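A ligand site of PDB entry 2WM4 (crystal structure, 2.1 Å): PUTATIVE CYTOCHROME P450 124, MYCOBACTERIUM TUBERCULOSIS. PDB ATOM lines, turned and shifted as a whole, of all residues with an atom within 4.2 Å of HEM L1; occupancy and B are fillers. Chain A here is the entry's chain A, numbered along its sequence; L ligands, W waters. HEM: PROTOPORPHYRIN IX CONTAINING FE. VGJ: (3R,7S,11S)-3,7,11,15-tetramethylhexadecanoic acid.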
ATOM      1  N   MET A 117      29.890  14.785   4.306  1.00  0.00           N
ATOM      2  CA  MET A 117      30.937  14.567   3.311  1.00  0.00           C
ATOM      3  C   MET A 117      31.554  15.857   2.781  1.00  0.00           C
ATOM      4  O   MET A 117      32.680  15.838   2.175  1.00  0.00           O
ATOM      5  CB  MET A 117      30.344  13.771   2.126  1.00  0.00           C
ATOM      6  CG  MET A 117      29.250  14.543   1.364  1.00  0.00           C
ATOM      7  SD  MET A 117      28.478  13.769  -0.103  1.00  0.00           S
ATOM      8  CE  MET A 117      27.829  12.366   0.608  1.00  0.00           C
ATOM      9  N   ILE A 118      30.867  16.992   2.998  1.00  0.00           N
ATOM     10  CA  ILE A 118      31.428  18.278   2.577  1.00  0.00           C
ATOM     11  C   ILE A 118      32.706  18.644   3.387  1.00  0.00           C
ATOM     12  O   ILE A 118      33.515  19.487   2.953  1.00  0.00           O
ATOM     13  CB  ILE A 118      30.389  19.423   2.621  1.00  0.00           C
ATOM     14  CG1 ILE A 118      30.831  20.523   1.677  1.00  0.00           C
ATOM     15  CG2 ILE A 118      30.187  19.964   4.111  1.00  0.00           C
ATOM     16  CD1 ILE A 118      29.750  21.610   1.372  1.00  0.00           C
ATOM     17  N   HIS A 125      34.769  10.593   1.079  1.00  0.00           N
ATOM     18  CA  HIS A 125      33.803  11.534   0.500  1.00  0.00           C
ATOM     19  C   HIS A 125      33.010  10.995  -0.684  1.00  0.00           C
ATOM     20  O   HIS A 125      31.771  11.167  -0.769  1.00  0.00           O
ATOM     21  CB  HIS A 125      34.516  12.823   0.125  1.00  0.00           C
ATOM     22  CG  HIS A 125      33.785  13.635  -0.900  1.00  0.00           C
ATOM     23  ND1 HIS A 125      34.080  13.593  -2.250  1.00  0.00           N
ATOM     24  CD2 HIS A 125      32.782  14.530  -0.753  1.00  0.00           C
ATOM     25  CE1 HIS A 125      33.302  14.449  -2.882  1.00  0.00           C
ATOM     26  NE2 HIS A 125      32.495  15.016  -1.992  1.00  0.00           N
ATOM     27  N   ARG A 129      29.191  10.296  -1.252  1.00  0.00           N
ATOM     28  CA  ARG A 129      28.479  11.018  -2.296  1.00  0.00           C
ATOM     29  C   ARG A 129      27.698  10.031  -3.245  1.00  0.00           C
ATOM     30  O   ARG A 129      26.549  10.320  -3.603  1.00  0.00           O
ATOM     31  CB  ARG A 129      29.416  12.018  -3.033  1.00  0.00           C
ATOM     32  CG  ARG A 129      28.727  12.805  -4.139  1.00  0.00           C
ATOM     33  CD  ARG A 129      29.667  13.813  -4.730  1.00  0.00           C
ATOM     34  NE  ARG A 129      29.222  14.443  -5.968  1.00  0.00           N
ATOM     35  CZ  ARG A 129      29.198  15.766  -6.186  1.00  0.00           C
ATOM     36  NH1 ARG A 129      29.533  16.634  -5.235  1.00  0.00           N
ATOM     37  NH2 ARG A 129      28.827  16.233  -7.388  1.00  0.00           N
ATOM     38  N   PHE A 136      20.689  13.205  -8.611  1.00  0.00           N
ATOM     39  CA  PHE A 136      21.011  14.584  -8.936  1.00  0.00           C
ATOM     40  C   PHE A 136      21.637  14.733 -10.347  1.00  0.00           C
ATOM     41  O   PHE A 136      21.909  15.850 -10.826  1.00  0.00           O
ATOM     42  CB  PHE A 136      21.957  15.141  -7.852  1.00  0.00           C
ATOM     43  CG  PHE A 136      21.307  15.328  -6.511  1.00  0.00           C
ATOM     44  CD1 PHE A 136      20.683  16.535  -6.193  1.00  0.00           C
ATOM     45  CD2 PHE A 136      21.311  14.300  -5.562  1.00  0.00           C
ATOM     46  CE1 PHE A 136      20.049  16.711  -4.966  1.00  0.00           C
ATOM     47  CE2 PHE A 136      20.677  14.452  -4.316  1.00  0.00           C
ATOM     48  CZ  PHE A 136      20.045  15.664  -4.009  1.00  0.00           C
ATOM     49  N   ILE A 183      13.372  19.907  -2.468  1.00  0.00           N
ATOM     50  CA  ILE A 183      14.320  19.084  -1.665  1.00  0.00           C
ATOM     51  C   ILE A 183      13.591  18.215  -0.606  1.00  0.00           C
ATOM     52  O   ILE A 183      13.865  17.036  -0.418  1.00  0.00           O
ATOM     53  CB  ILE A 183      15.552  19.927  -1.020  1.00  0.00           C
ATOM     54  CG1 ILE A 183      16.655  18.989  -0.498  1.00  0.00           C
ATOM     55  CG2 ILE A 183      15.091  20.872   0.127  1.00  0.00           C
ATOM     56  CD1 ILE A 183      17.311  18.137  -1.560  1.00  0.00           C
ATOM     57  N   LEU A 270      22.990  18.307   5.620  1.00  0.00           N
ATOM     58  CA  LEU A 270      23.702  18.878   4.479  1.00  0.00           C
ATOM     59  C   LEU A 270      22.737  19.084   3.298  1.00  0.00           C
ATOM     60  O   LEU A 270      22.659  20.192   2.723  1.00  0.00           O
ATOM     61  CB  LEU A 270      24.865  17.967   4.068  1.00  0.00           C
ATOM     62  CG  LEU A 270      25.520  18.246   2.716  1.00  0.00           C
ATOM     63  CD1 LEU A 270      26.269  19.614   2.667  1.00  0.00           C
ATOM     64  CD2 LEU A 270      26.439  17.061   2.410  1.00  0.00           C
ATOM     65  N   LEU A 271      21.995  18.020   2.951  1.00  0.00           N
ATOM     66  CA  LEU A 271      21.064  18.110   1.783  1.00  0.00           C
ATOM     67  C   LEU A 271      20.012  19.206   1.930  1.00  0.00           C
ATOM     68  O   LEU A 271      19.826  20.053   1.064  1.00  0.00           O
ATOM     69  CB  LEU A 271      20.402  16.805   1.537  1.00  0.00           C
ATOM     70  CG  LEU A 271      21.406  15.781   0.965  1.00  0.00           C
ATOM     71  CD1 LEU A 271      20.823  14.386   0.987  1.00  0.00           C
ATOM     72  CD2 LEU A 271      21.958  16.123  -0.459  1.00  0.00           C
ATOM     73  N   ALA A 274      21.709  22.837   2.174  1.00  0.00           N
ATOM     74  CA  ALA A 274      22.180  23.240   0.862  1.00  0.00           C
ATOM     75  C   ALA A 274      20.945  23.456  -0.019  1.00  0.00           C
ATOM     76  O   ALA A 274      20.832  24.493  -0.659  1.00  0.00           O
ATOM     77  CB  ALA A 274      23.139  22.193   0.256  1.00  0.00           C
ATOM     78  N   GLY A 275      19.966  22.538   0.004  1.00  0.00           N
ATOM     79  CA  GLY A 275      18.780  22.734  -0.867  1.00  0.00           C
ATOM     80  C   GLY A 275      17.994  24.007  -0.536  1.00  0.00           C
ATOM     81  O   GLY A 275      17.409  24.641  -1.425  1.00  0.00           O
ATOM     82  N   THR A 278      20.182  28.426  -0.851  1.00  0.00           N
ATOM     83  CA  THR A 278      21.082  28.573  -1.948  1.00  0.00           C
ATOM     84  C   THR A 278      20.342  29.107  -3.215  1.00  0.00           C
ATOM     85  O   THR A 278      20.430  30.305  -3.560  1.00  0.00           O
ATOM     86  CB  THR A 278      21.692  27.166  -2.016  1.00  0.00           C
ATOM     87  OG1 THR A 278      23.126  27.157  -1.870  1.00  0.00           O
ATOM     88  CG2 THR A 278      21.095  26.373  -2.996  1.00  0.00           C
ATOM     89  N   THR A 279      19.580  28.241  -3.881  1.00  0.00           N
ATOM     90  CA  THR A 279      18.784  28.671  -5.039  1.00  0.00           C
ATOM     91  C   THR A 279      17.720  29.751  -4.814  1.00  0.00           C
ATOM     92  O   THR A 279      17.544  30.654  -5.670  1.00  0.00           O
ATOM     93  CB  THR A 279      18.405  27.528  -5.992  1.00  0.00           C
ATOM     94  OG1 THR A 279      17.119  27.748  -6.602  1.00  0.00           O
ATOM     95  CG2 THR A 279      18.511  26.207  -5.349  1.00  0.00           C
ATOM     96  N   ALA A 282      19.722  32.836  -5.491  1.00  0.00           N
ATOM     97  CA  ALA A 282      19.867  33.023  -6.960  1.00  0.00           C
ATOM     98  C   ALA A 282      18.588  33.601  -7.556  1.00  0.00           C
ATOM     99  O   ALA A 282      18.626  34.582  -8.330  1.00  0.00           O
ATOM    100  CB  ALA A 282      20.233  31.692  -7.691  1.00  0.00           C
ATOM    101  N   VAL A 316      23.349  33.088 -11.759  1.00  0.00           N
ATOM    102  CA  VAL A 316      24.175  32.448 -10.716  1.00  0.00           C
ATOM    103  C   VAL A 316      25.489  33.215 -10.487  1.00  0.00           C
ATOM    104  O   VAL A 316      25.873  33.484  -9.334  1.00  0.00           O
ATOM    105  CB  VAL A 316      24.461  30.933 -10.994  1.00  0.00           C
ATOM    106  CG1 VAL A 316      25.468  30.391 -10.045  1.00  0.00           C
ATOM    107  CG2 VAL A 316      23.178  30.165 -10.837  1.00  0.00           C
ATOM    108  N   PRO A 321      25.551  32.909  -4.841  1.00  0.00           N
ATOM    109  CA  PRO A 321      24.778  32.681  -3.594  1.00  0.00           C
ATOM    110  C   PRO A 321      25.596  32.234  -2.375  1.00  0.00           C
ATOM    111  O   PRO A 321      25.257  32.574  -1.231  1.00  0.00           O
ATOM    112  CB  PRO A 321      23.777  31.588  -3.992  1.00  0.00           C
ATOM    113  CG  PRO A 321      23.460  31.955  -5.494  1.00  0.00           C
ATOM    114  CD  PRO A 321      24.914  32.224  -5.997  1.00  0.00           C
ATOM    115  N   VAL A 322      26.654  31.450  -2.654  1.00  0.00           N
ATOM    116  CA  VAL A 322      27.633  30.987  -1.684  1.00  0.00           C
ATOM    117  C   VAL A 322      28.876  31.818  -1.877  1.00  0.00           C
ATOM    118  O   VAL A 322      29.545  31.783  -2.930  1.00  0.00           O
ATOM    119  CB  VAL A 322      28.002  29.485  -1.859  1.00  0.00           C
ATOM    120  CG1 VAL A 322      29.077  29.060  -0.781  1.00  0.00           C
ATOM    121  CG2 VAL A 322      26.760  28.597  -1.741  1.00  0.00           C
ATOM    122  N   MET A 325      34.109  29.184   0.282  1.00  0.00           N
ATOM    123  CA  MET A 325      34.291  27.968   1.070  1.00  0.00           C
ATOM    124  C   MET A 325      35.725  28.005   1.631  1.00  0.00           C
ATOM    125  O   MET A 325      36.608  28.576   1.018  1.00  0.00           O
ATOM    126  CB  MET A 325      34.136  26.679   0.217  1.00  0.00           C
ATOM    127  CG  MET A 325      32.678  26.362  -0.133  1.00  0.00           C
ATOM    128  SD  MET A 325      31.832  25.664   1.299  1.00  0.00           S
ATOM    129  CE  MET A 325      30.167  25.444   0.648  1.00  0.00           C
ATOM    130  N   ARG A 327      39.262  25.849   2.904  1.00  0.00           N
ATOM    131  CA  ARG A 327      40.091  24.632   2.835  1.00  0.00           C
ATOM    132  C   ARG A 327      41.179  24.743   3.930  1.00  0.00           C
ATOM    133  O   ARG A 327      41.300  25.782   4.545  1.00  0.00           O
ATOM    134  CB  ARG A 327      40.737  24.478   1.436  1.00  0.00           C
ATOM    135  CG  ARG A 327      39.740  24.375   0.274  1.00  0.00           C
ATOM    136  CD  ARG A 327      38.920  23.095   0.421  1.00  0.00           C
ATOM    137  NE  ARG A 327      38.149  22.755  -0.781  1.00  0.00           N
ATOM    138  CZ  ARG A 327      36.828  22.913  -0.905  1.00  0.00           C
ATOM    139  NH1 ARG A 327      36.125  23.460   0.114  1.00  0.00           N
ATOM    140  NH2 ARG A 327      36.204  22.512  -2.030  1.00  0.00           N
ATOM    141  N   TYR A 350      34.365  32.911  -3.882  1.00  0.00           N
ATOM    142  CA  TYR A 350      33.644  32.808  -5.181  1.00  0.00           C
ATOM    143  C   TYR A 350      33.074  34.127  -5.732  1.00  0.00           C
ATOM    144  O   TYR A 350      33.067  34.371  -6.932  1.00  0.00           O
ATOM    145  CB  TYR A 350      32.524  31.759  -5.140  1.00  0.00           C
ATOM    146  CG  TYR A 350      32.993  30.404  -4.642  1.00  0.00           C
ATOM    147  CD1 TYR A 350      34.030  29.693  -5.310  1.00  0.00           C
ATOM    148  CD2 TYR A 350      32.434  29.855  -3.514  1.00  0.00           C
ATOM    149  CE1 TYR A 350      34.467  28.470  -4.820  1.00  0.00           C
ATOM    150  CE2 TYR A 350      32.823  28.614  -3.034  1.00  0.00           C
ATOM    151  CZ  TYR A 350      33.840  27.940  -3.687  1.00  0.00           C
ATOM    152  OH  TYR A 350      34.180  26.724  -3.175  1.00  0.00           O
ATOM    153  N   GLY A 377      30.098  29.961  -9.329  1.00  0.00           N
ATOM    154  CA  GLY A 377      29.026  30.026  -8.340  1.00  0.00           C
ATOM    155  C   GLY A 377      28.792  28.665  -7.701  1.00  0.00           C
ATOM    156  O   GLY A 377      28.358  28.603  -6.532  1.00  0.00           O
ATOM    157  N   PHE A 378      29.078  27.578  -8.445  1.00  0.00           N
ATOM    158  CA  PHE A 378      28.968  26.182  -7.948  1.00  0.00           C
ATOM    159  C   PHE A 378      30.333  25.660  -7.506  1.00  0.00           C
ATOM    160  O   PHE A 378      30.472  24.465  -7.279  1.00  0.00           O
ATOM    161  CB  PHE A 378      28.377  25.244  -9.022  1.00  0.00           C
ATOM    162  CG  PHE A 378      26.965  25.609  -9.425  1.00  0.00           C
ATOM    163  CD1 PHE A 378      25.905  25.469  -8.478  1.00  0.00           C
ATOM    164  CD2 PHE A 378      26.679  26.090 -10.705  1.00  0.00           C
ATOM    165  CE1 PHE A 378      24.559  25.809  -8.810  1.00  0.00           C
ATOM    166  CE2 PHE A 378      25.318  26.419 -11.070  1.00  0.00           C
ATOM    167  CZ  PHE A 378      24.254  26.314 -10.093  1.00  0.00           C
ATOM    168  N   GLY A 379      31.289  26.580  -7.309  1.00  0.00           N
ATOM    169  CA  GLY A 379      32.647  26.280  -6.804  1.00  0.00           C
ATOM    170  C   GLY A 379      33.558  26.096  -8.011  1.00  0.00           C
ATOM    171  O   GLY A 379      33.097  26.298  -9.156  1.00  0.00           O
ATOM    172  N   GLY A 380      34.807  25.655  -7.786  1.00  0.00           N
ATOM    173  CA  GLY A 380      35.802  25.670  -8.839  1.00  0.00           C
ATOM    174  C   GLY A 380      35.912  24.340  -9.582  1.00  0.00           C
ATOM    175  O   GLY A 380      36.785  24.145 -10.421  1.00  0.00           O
ATOM    176  N   ALA A 383      36.285  17.556  -6.867  1.00  0.00           N
ATOM    177  CA  ALA A 383      35.664  16.545  -6.046  1.00  0.00           C
ATOM    178  C   ALA A 383      34.369  16.972  -5.352  1.00  0.00           C
ATOM    179  O   ALA A 383      33.481  16.142  -5.158  1.00  0.00           O
ATOM    180  CB  ALA A 383      36.668  16.027  -4.997  1.00  0.00           C
ATOM    181  N   HIS A 384      34.246  18.223  -4.934  1.00  0.00           N
ATOM    182  CA  HIS A 384      33.037  18.635  -4.190  1.00  0.00           C
ATOM    183  C   HIS A 384      32.109  19.462  -5.054  1.00  0.00           C
ATOM    184  O   HIS A 384      31.273  20.188  -4.506  1.00  0.00           O
ATOM    185  CB  HIS A 384      33.439  19.443  -2.898  1.00  0.00           C
ATOM    186  CG  HIS A 384      34.132  18.594  -1.890  1.00  0.00           C
ATOM    187  ND1 HIS A 384      33.457  17.880  -0.924  1.00  0.00           N
ATOM    188  CD2 HIS A 384      35.429  18.246  -1.772  1.00  0.00           C
ATOM    189  CE1 HIS A 384      34.306  17.176  -0.217  1.00  0.00           C
ATOM    190  NE2 HIS A 384      35.520  17.374  -0.710  1.00  0.00           N
ATOM    191  N   PHE A 385      32.284  19.401  -6.368  1.00  0.00           N
ATOM    192  CA  PHE A 385      31.414  20.222  -7.271  1.00  0.00           C
ATOM    193  C   PHE A 385      29.958  20.124  -6.857  1.00  0.00           C
ATOM    194  O   PHE A 385      29.468  19.025  -6.583  1.00  0.00           O
ATOM    195  CB  PHE A 385      31.533  19.830  -8.748  1.00  0.00           C
ATOM    196  CG  PHE A 385      30.641  20.655  -9.613  1.00  0.00           C
ATOM    197  CD1 PHE A 385      30.923  22.005  -9.844  1.00  0.00           C
ATOM    198  CD2 PHE A 385      29.471  20.090 -10.182  1.00  0.00           C
ATOM    199  CE1 PHE A 385      30.083  22.793 -10.623  1.00  0.00           C
ATOM    200  CE2 PHE A 385      28.650  20.870 -10.970  1.00  0.00           C
ATOM    201  CZ  PHE A 385      28.948  22.210 -11.180  1.00  0.00           C
ATOM    202  N   CYS A 386      29.284  21.248  -6.771  1.00  0.00           N
ATOM    203  CA  CYS A 386      27.973  21.279  -6.159  1.00  0.00           C
ATOM    204  C   CYS A 386      27.101  20.111  -6.636  1.00  0.00           C
ATOM    205  O   CYS A 386      26.838  19.929  -7.850  1.00  0.00           O
ATOM    206  CB  CYS A 386      27.297  22.579  -6.542  1.00  0.00           C
ATOM    207  SG  CYS A 386      25.516  22.549  -6.188  1.00  0.00           S
ATOM    208  N   LEU A 387      26.620  19.321  -5.694  1.00  0.00           N
ATOM    209  CA  LEU A 387      25.880  18.155  -6.110  1.00  0.00           C
ATOM    210  C   LEU A 387      24.545  18.568  -6.714  1.00  0.00           C
ATOM    211  O   LEU A 387      24.051  17.862  -7.588  1.00  0.00           O
ATOM    212  CB  LEU A 387      25.666  17.176  -4.940  1.00  0.00           C
ATOM    213  CG  LEU A 387      24.748  15.937  -5.128  1.00  0.00           C
ATOM    214  CD1 LEU A 387      25.351  14.979  -6.152  1.00  0.00           C
ATOM    215  CD2 LEU A 387      24.554  15.212  -3.764  1.00  0.00           C
ATOM    216  N   GLY A 388      23.947  19.661  -6.213  1.00  0.00           N
ATOM    217  CA  GLY A 388      22.681  20.154  -6.688  1.00  0.00           C
ATOM    218  C   GLY A 388      22.740  21.069  -7.903  1.00  0.00           C
ATOM    219  O   GLY A 388      21.722  21.668  -8.290  1.00  0.00           O
ATOM    220  N   LEU A 391      19.881  20.314 -10.593  1.00  0.00           N
ATOM    221  CA  LEU A 391      18.677  20.699  -9.884  1.00  0.00           C
ATOM    222  C   LEU A 391      18.463  22.200  -9.687  1.00  0.00           C
ATOM    223  O   LEU A 391      17.378  22.709  -9.998  1.00  0.00           O
ATOM    224  CB  LEU A 391      18.572  19.987  -8.517  1.00  0.00           C
ATOM    225  CG  LEU A 391      17.340  20.316  -7.651  1.00  0.00           C
ATOM    226  CD1 LEU A 391      16.085  19.763  -8.359  1.00  0.00           C
ATOM    227  CD2 LEU A 391      17.477  19.717  -6.236  1.00  0.00           C
ATOM    228  N   ALA A 392      19.466  22.908  -9.169  1.00  0.00           N
ATOM    229  CA  ALA A 392      19.391  24.374  -9.028  1.00  0.00           C
ATOM    230  C   ALA A 392      19.088  25.111 -10.384  1.00  0.00           C
ATOM    231  O   ALA A 392      18.207  25.976 -10.490  1.00  0.00           O
ATOM    232  CB  ALA A 392      20.741  24.869  -8.394  1.00  0.00           C
ATOM    233  N   GLU A 395      15.587  24.512 -11.236  1.00  0.00           N
ATOM    234  CA  GLU A 395      14.718  25.291 -10.350  1.00  0.00           C
ATOM    235  C   GLU A 395      14.708  26.747 -10.840  1.00  0.00           C
ATOM    236  O   GLU A 395      13.671  27.381 -10.879  1.00  0.00           O
ATOM    237  CB  GLU A 395      15.140  25.209  -8.879  1.00  0.00           C
ATOM    238  CG  GLU A 395      14.965  23.847  -8.238  1.00  0.00           C
ATOM    239  CD  GLU A 395      15.630  23.734  -6.846  1.00  0.00           C
ATOM    240  OE1 GLU A 395      16.572  24.560  -6.558  1.00  0.00           O
ATOM    241  OE2 GLU A 395      15.201  22.829  -6.057  1.00  0.00           O
ATOM    242  N   ILE A 396      15.860  27.272 -11.215  1.00  0.00           N
ATOM    243  CA  ILE A 396      15.948  28.673 -11.539  1.00  0.00           C
ATOM    244  C   ILE A 396      15.186  28.903 -12.828  1.00  0.00           C
ATOM    245  O   ILE A 396      14.415  29.834 -12.941  1.00  0.00           O
ATOM    246  CB  ILE A 396      17.421  29.201 -11.625  1.00  0.00           C
ATOM    247  CG1 ILE A 396      18.111  28.992 -10.260  1.00  0.00           C
ATOM    248  CG2 ILE A 396      17.428  30.674 -12.024  1.00  0.00           C
ATOM    249  CD1 ILE A 396      19.694  29.093 -10.244  1.00  0.00           C
HETATM  250  CHA HEM L   1      28.316  22.033  -2.578  1.00  0.00           C
HETATM  251  CHB HEM L   1      26.846  26.335  -4.379  1.00  0.00           C
HETATM  252  CHC HEM L   1      22.264  24.585  -4.840  1.00  0.00           C
HETATM  253  CHD HEM L   1      23.618  20.496  -2.607  1.00  0.00           C
HETATM  254  C1A HEM L   1      28.317  23.356  -3.045  1.00  0.00           C
HETATM  255  C2A HEM L   1      29.484  24.241  -3.086  1.00  0.00           C
HETATM  256  C3A HEM L   1      29.079  25.433  -3.616  1.00  0.00           C
HETATM  257  C4A HEM L   1      27.655  25.337  -3.868  1.00  0.00           C
HETATM  258  CMA HEM L   1      29.929  26.685  -3.867  1.00  0.00           C
HETATM  259  CAA HEM L   1      30.922  23.818  -2.691  1.00  0.00           C
HETATM  260  CBA HEM L   1      31.660  23.368  -3.998  1.00  0.00           C
HETATM  261  CGA HEM L   1      33.149  23.027  -3.910  1.00  0.00           C
HETATM  262  O1A HEM L   1      33.648  22.818  -2.790  1.00  0.00           O
HETATM  263  O2A HEM L   1      33.905  22.971  -4.936  1.00  0.00           O
HETATM  264  C1B HEM L   1      25.475  26.150  -4.715  1.00  0.00           C
HETATM  265  C2B HEM L   1      24.690  27.100  -5.439  1.00  0.00           C
HETATM  266  C3B HEM L   1      23.448  26.637  -5.606  1.00  0.00           C
HETATM  267  C4B HEM L   1      23.389  25.363  -4.908  1.00  0.00           C
HETATM  268  CMB HEM L   1      25.237  28.439  -5.958  1.00  0.00           C
HETATM  269  CAB HEM L   1      22.233  27.306  -6.295  1.00  0.00           C
HETATM  270  CBB HEM L   1      22.352  28.295  -7.205  1.00  0.00           C
HETATM  271  C1C HEM L   1      22.238  23.344  -4.246  1.00  0.00           C
HETATM  272  C2C HEM L   1      21.066  22.499  -4.135  1.00  0.00           C
HETATM  273  C3C HEM L   1      21.444  21.397  -3.502  1.00  0.00           C
HETATM  274  C4C HEM L   1      22.861  21.474  -3.225  1.00  0.00           C
HETATM  275  CMC HEM L   1      19.647  22.888  -4.608  1.00  0.00           C
HETATM  276  CAC HEM L   1      20.541  20.227  -3.161  1.00  0.00           C
HETATM  277  CBC HEM L   1      20.683  19.510  -2.055  1.00  0.00           C
HETATM  278  C1D HEM L   1      25.010  20.561  -2.431  1.00  0.00           C
HETATM  279  C2D HEM L   1      25.784  19.527  -1.786  1.00  0.00           C
HETATM  280  C3D HEM L   1      27.237  19.958  -1.769  1.00  0.00           C
HETATM  281  C4D HEM L   1      27.216  21.258  -2.402  1.00  0.00           C
HETATM  282  CMD HEM L   1      25.276  18.172  -1.238  1.00  0.00           C
HETATM  283  CAD HEM L   1      28.389  19.083  -1.226  1.00  0.00           C
HETATM  284  CBD HEM L   1      28.946  18.246  -2.424  1.00  0.00           C
HETATM  285  CGD HEM L   1      30.172  17.430  -2.017  1.00  0.00           C
HETATM  286  O1D HEM L   1      30.738  17.687  -0.887  1.00  0.00           O
HETATM  287  O2D HEM L   1      30.612  16.542  -2.804  1.00  0.00           O
HETATM  288  NA  HEM L   1      27.229  24.062  -3.526  1.00  0.00           N
HETATM  289  NB  HEM L   1      24.649  25.100  -4.376  1.00  0.00           N
HETATM  290  NC  HEM L   1      23.317  22.678  -3.728  1.00  0.00           N
HETATM  291  ND  HEM L   1      25.886  21.578  -2.795  1.00  0.00           N
HETATM  292 FE   HEM L   1      25.333  23.247  -3.949  1.00  0.00          FE
HETATM  293  O1  VGJ L   2      32.750  32.972  11.248  1.00  0.00           O
HETATM  294  C15 VGJ L   2      32.163  31.966  11.777  1.00  0.00           C
HETATM  295  O2  VGJ L   2      32.160  31.846  13.023  1.00  0.00           O
HETATM  296  C14 VGJ L   2      31.480  30.876  10.912  1.00  0.00           C
HETATM  297  C13 VGJ L   2      29.937  30.646  11.043  1.00  0.00           C
HETATM  298  C16 VGJ L   2      29.465  30.561  12.498  1.00  0.00           C
HETATM  299  C12 VGJ L   2      29.373  29.464  10.195  1.00  0.00           C
HETATM  300  C11 VGJ L   2      28.614  28.327  10.957  1.00  0.00           C
HETATM  301  C10 VGJ L   2      27.548  27.484  10.221  1.00  0.00           C
HETATM  302  C9  VGJ L   2      27.953  26.036   9.853  1.00  0.00           C
HETATM  303  C17 VGJ L   2      27.825  25.052  11.022  1.00  0.00           C
HETATM  304  C8  VGJ L   2      27.168  25.549   8.620  1.00  0.00           C
HETATM  305  C7  VGJ L   2      27.588  24.197   7.979  1.00  0.00           C
HETATM  306  C6  VGJ L   2      27.348  24.163   6.445  1.00  0.00           C
HETATM  307  C5  VGJ L   2      26.627  22.954   5.822  1.00  0.00           C
HETATM  308  C18 VGJ L   2      25.496  22.442   6.684  1.00  0.00           C
HETATM  309  C4  VGJ L   2      25.915  23.258   4.500  1.00  0.00           C
HETATM  310  C3  VGJ L   2      26.530  24.210   3.465  1.00  0.00           C
HETATM  311  C2  VGJ L   2      25.927  23.914   2.096  1.00  0.00           C
HETATM  312  C1  VGJ L   2      26.306  24.943   1.050  1.00  0.00           C
HETATM  313  C19 VGJ L   2      25.452  26.207   1.182  1.00  0.00           C
HETATM  314  C20 VGJ L   2      26.291  24.367  -0.363  1.00  0.00           C
HETATM  315  O   HOH W   1      35.584  20.817  -5.484  1.00  0.00           O
HETATM  316  O   HOH W   2      33.002  23.246  -7.397  1.00  0.00           O
HETATM  317  O   HOH W   3      35.374  25.183  -4.920  1.00  0.00           O
HETATM  318  O   HOH W   4      33.344  23.037   0.022  1.00  0.00           O
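The side-chain sulfur (SG) of Cys 386 binds an iron atom (FE) of HEM L1 (2.4 Å).
An oxygen (O2D) of HEM L1 lies within hydrogen-bond range of a ring nitrogen (NE2) of His 125, 2.6 Å away.
NH1 of Arg 129 lies within salt-bridge range of O2D of HEM L1 (2.7 Å).
The guanidinium group (NH2) of Arg 327 is in salt-bridge range of an oxygen (O1A) of HEM L1 (2.7 Å).
An oxygen (O1D) of HEM L1 is in hydrogen-bond range of a ring nitrogen (ND1) of His 384 (2.7 Å).
Water W2 lies within hydrogen-bond range of O2A of HEM L1 (2.6 Å), O of Phe 378 (2.8 Å) and N of Gly 380 (3.0 Å).
Water W3 lies within hydrogen-bond range of the side-chain hydroxyl (OH) of Tyr 350 (2.6 Å), an oxygen (O2A) of HEM L1 (2.7 Å) and the backbone NH (N) of Gly 380 (3.0 Å).
Water W1 bridges an oxygen (O2A) of HEM L1 and the backbone NH of His 384.
Water W4 lies within hydrogen-bond range of the guanidinium group of Arg 327 (2.8 Å), an oxygen (O1A) of HEM L1 (2.8 Å) and the side-chain sulfur of Met 325 (3.3 Å).
The backbone NH of Cys 386 lies within hydrogen-bond range of the backbone carbonyl oxygen of Phe 378 (3.5 Å).
N of Gly 388 lies close to SG of Cys 386 (3.3 Å).
A ring nitrogen (ND1) of His 384 sits at hydrogen-bond distance from a ring nitrogen (NE2) of His 125 (3.2 Å).
The side-chain sulfur (SD) of Met 117 lies close to the backbone NH (N) of Arg 129 (3.7 Å).
NH1 of Arg 129 lies within hydrogen-bond range of O of Phe 385.
The side-chain hydroxyl of Thr 279 sits close to the side-chain carboxylate of Glu 395 (3.2 Å).
Ile 118 touches HEM L1.
Phe 136 touches HEM L1.
CD1 of Ile 183 touches CBC of HEM L1 (3.7 Å).
CG of Leu 270 touches CMD of HEM L1, 3.96 Å away.
Leu 271 touches HEM L1 (O to CBC, 3.3 Å).
CB of Ala 274 touches CHD of HEM L1, at 3.4 Å.
N of Gly 275 touches CBC of HEM L1, at 3.7 Å.
Thr 278 touches HEM L1 (CG2 to CHC, 2.8 Å).
CG2 of Thr 279 touches CMC of HEM L1 (3.6 Å).
Pro 321 touches HEM L1.
Val 322 touches HEM L1 (CG2 to CHB, 3.5 Å).
Met 325 touches HEM L1 (CE to CAA, 3.8 Å).
Tyr 350 touches HEM L1 (CE2 to CMA, 3.6 Å).
Gly 377 touches HEM L1.
CE1 of Phe 378 touches C3B of HEM L1, 3.5 Å away.
Gly 379 touches HEM L1.
Ala 383 touches HEM L1 (O to O2D, 3.7 Å).
Leu 387 touches HEM L1 (N to ND, 3.7 Å).
Gly 388 touches HEM L1 (CA to C3C, 3.6 Å).
CB of Ala 392 touches CAB of HEM L1, 3.5 Å away.
Hydrophobic or aromatic side chains that line HEM L1: Ile 118, His 125, Phe 136, Ile 183, Leu 270, Leu 271, Ala 274, Pro 321, Val 322, Met 325, Tyr 350, Phe 378, His 384, Leu 387 and Ala 392.
25 residues have an atom within 4 Å of HEM L1: Ile 118, His 125, Arg 129, Phe 136, Ile 183, Leu 270, Leu 271, Ala 274, Gly 275, Thr 278, Thr 279, Pro 321, Val 322, Met 325, Arg 327, Tyr 350, Gly 377, Phe 378, Gly 379, Ala 383, His 384, Cys 386, Leu 387, Gly 388 and Ala 392.
The nearest printed residue that does not touch HEM L1 is Glu 395 (4.01 Å).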
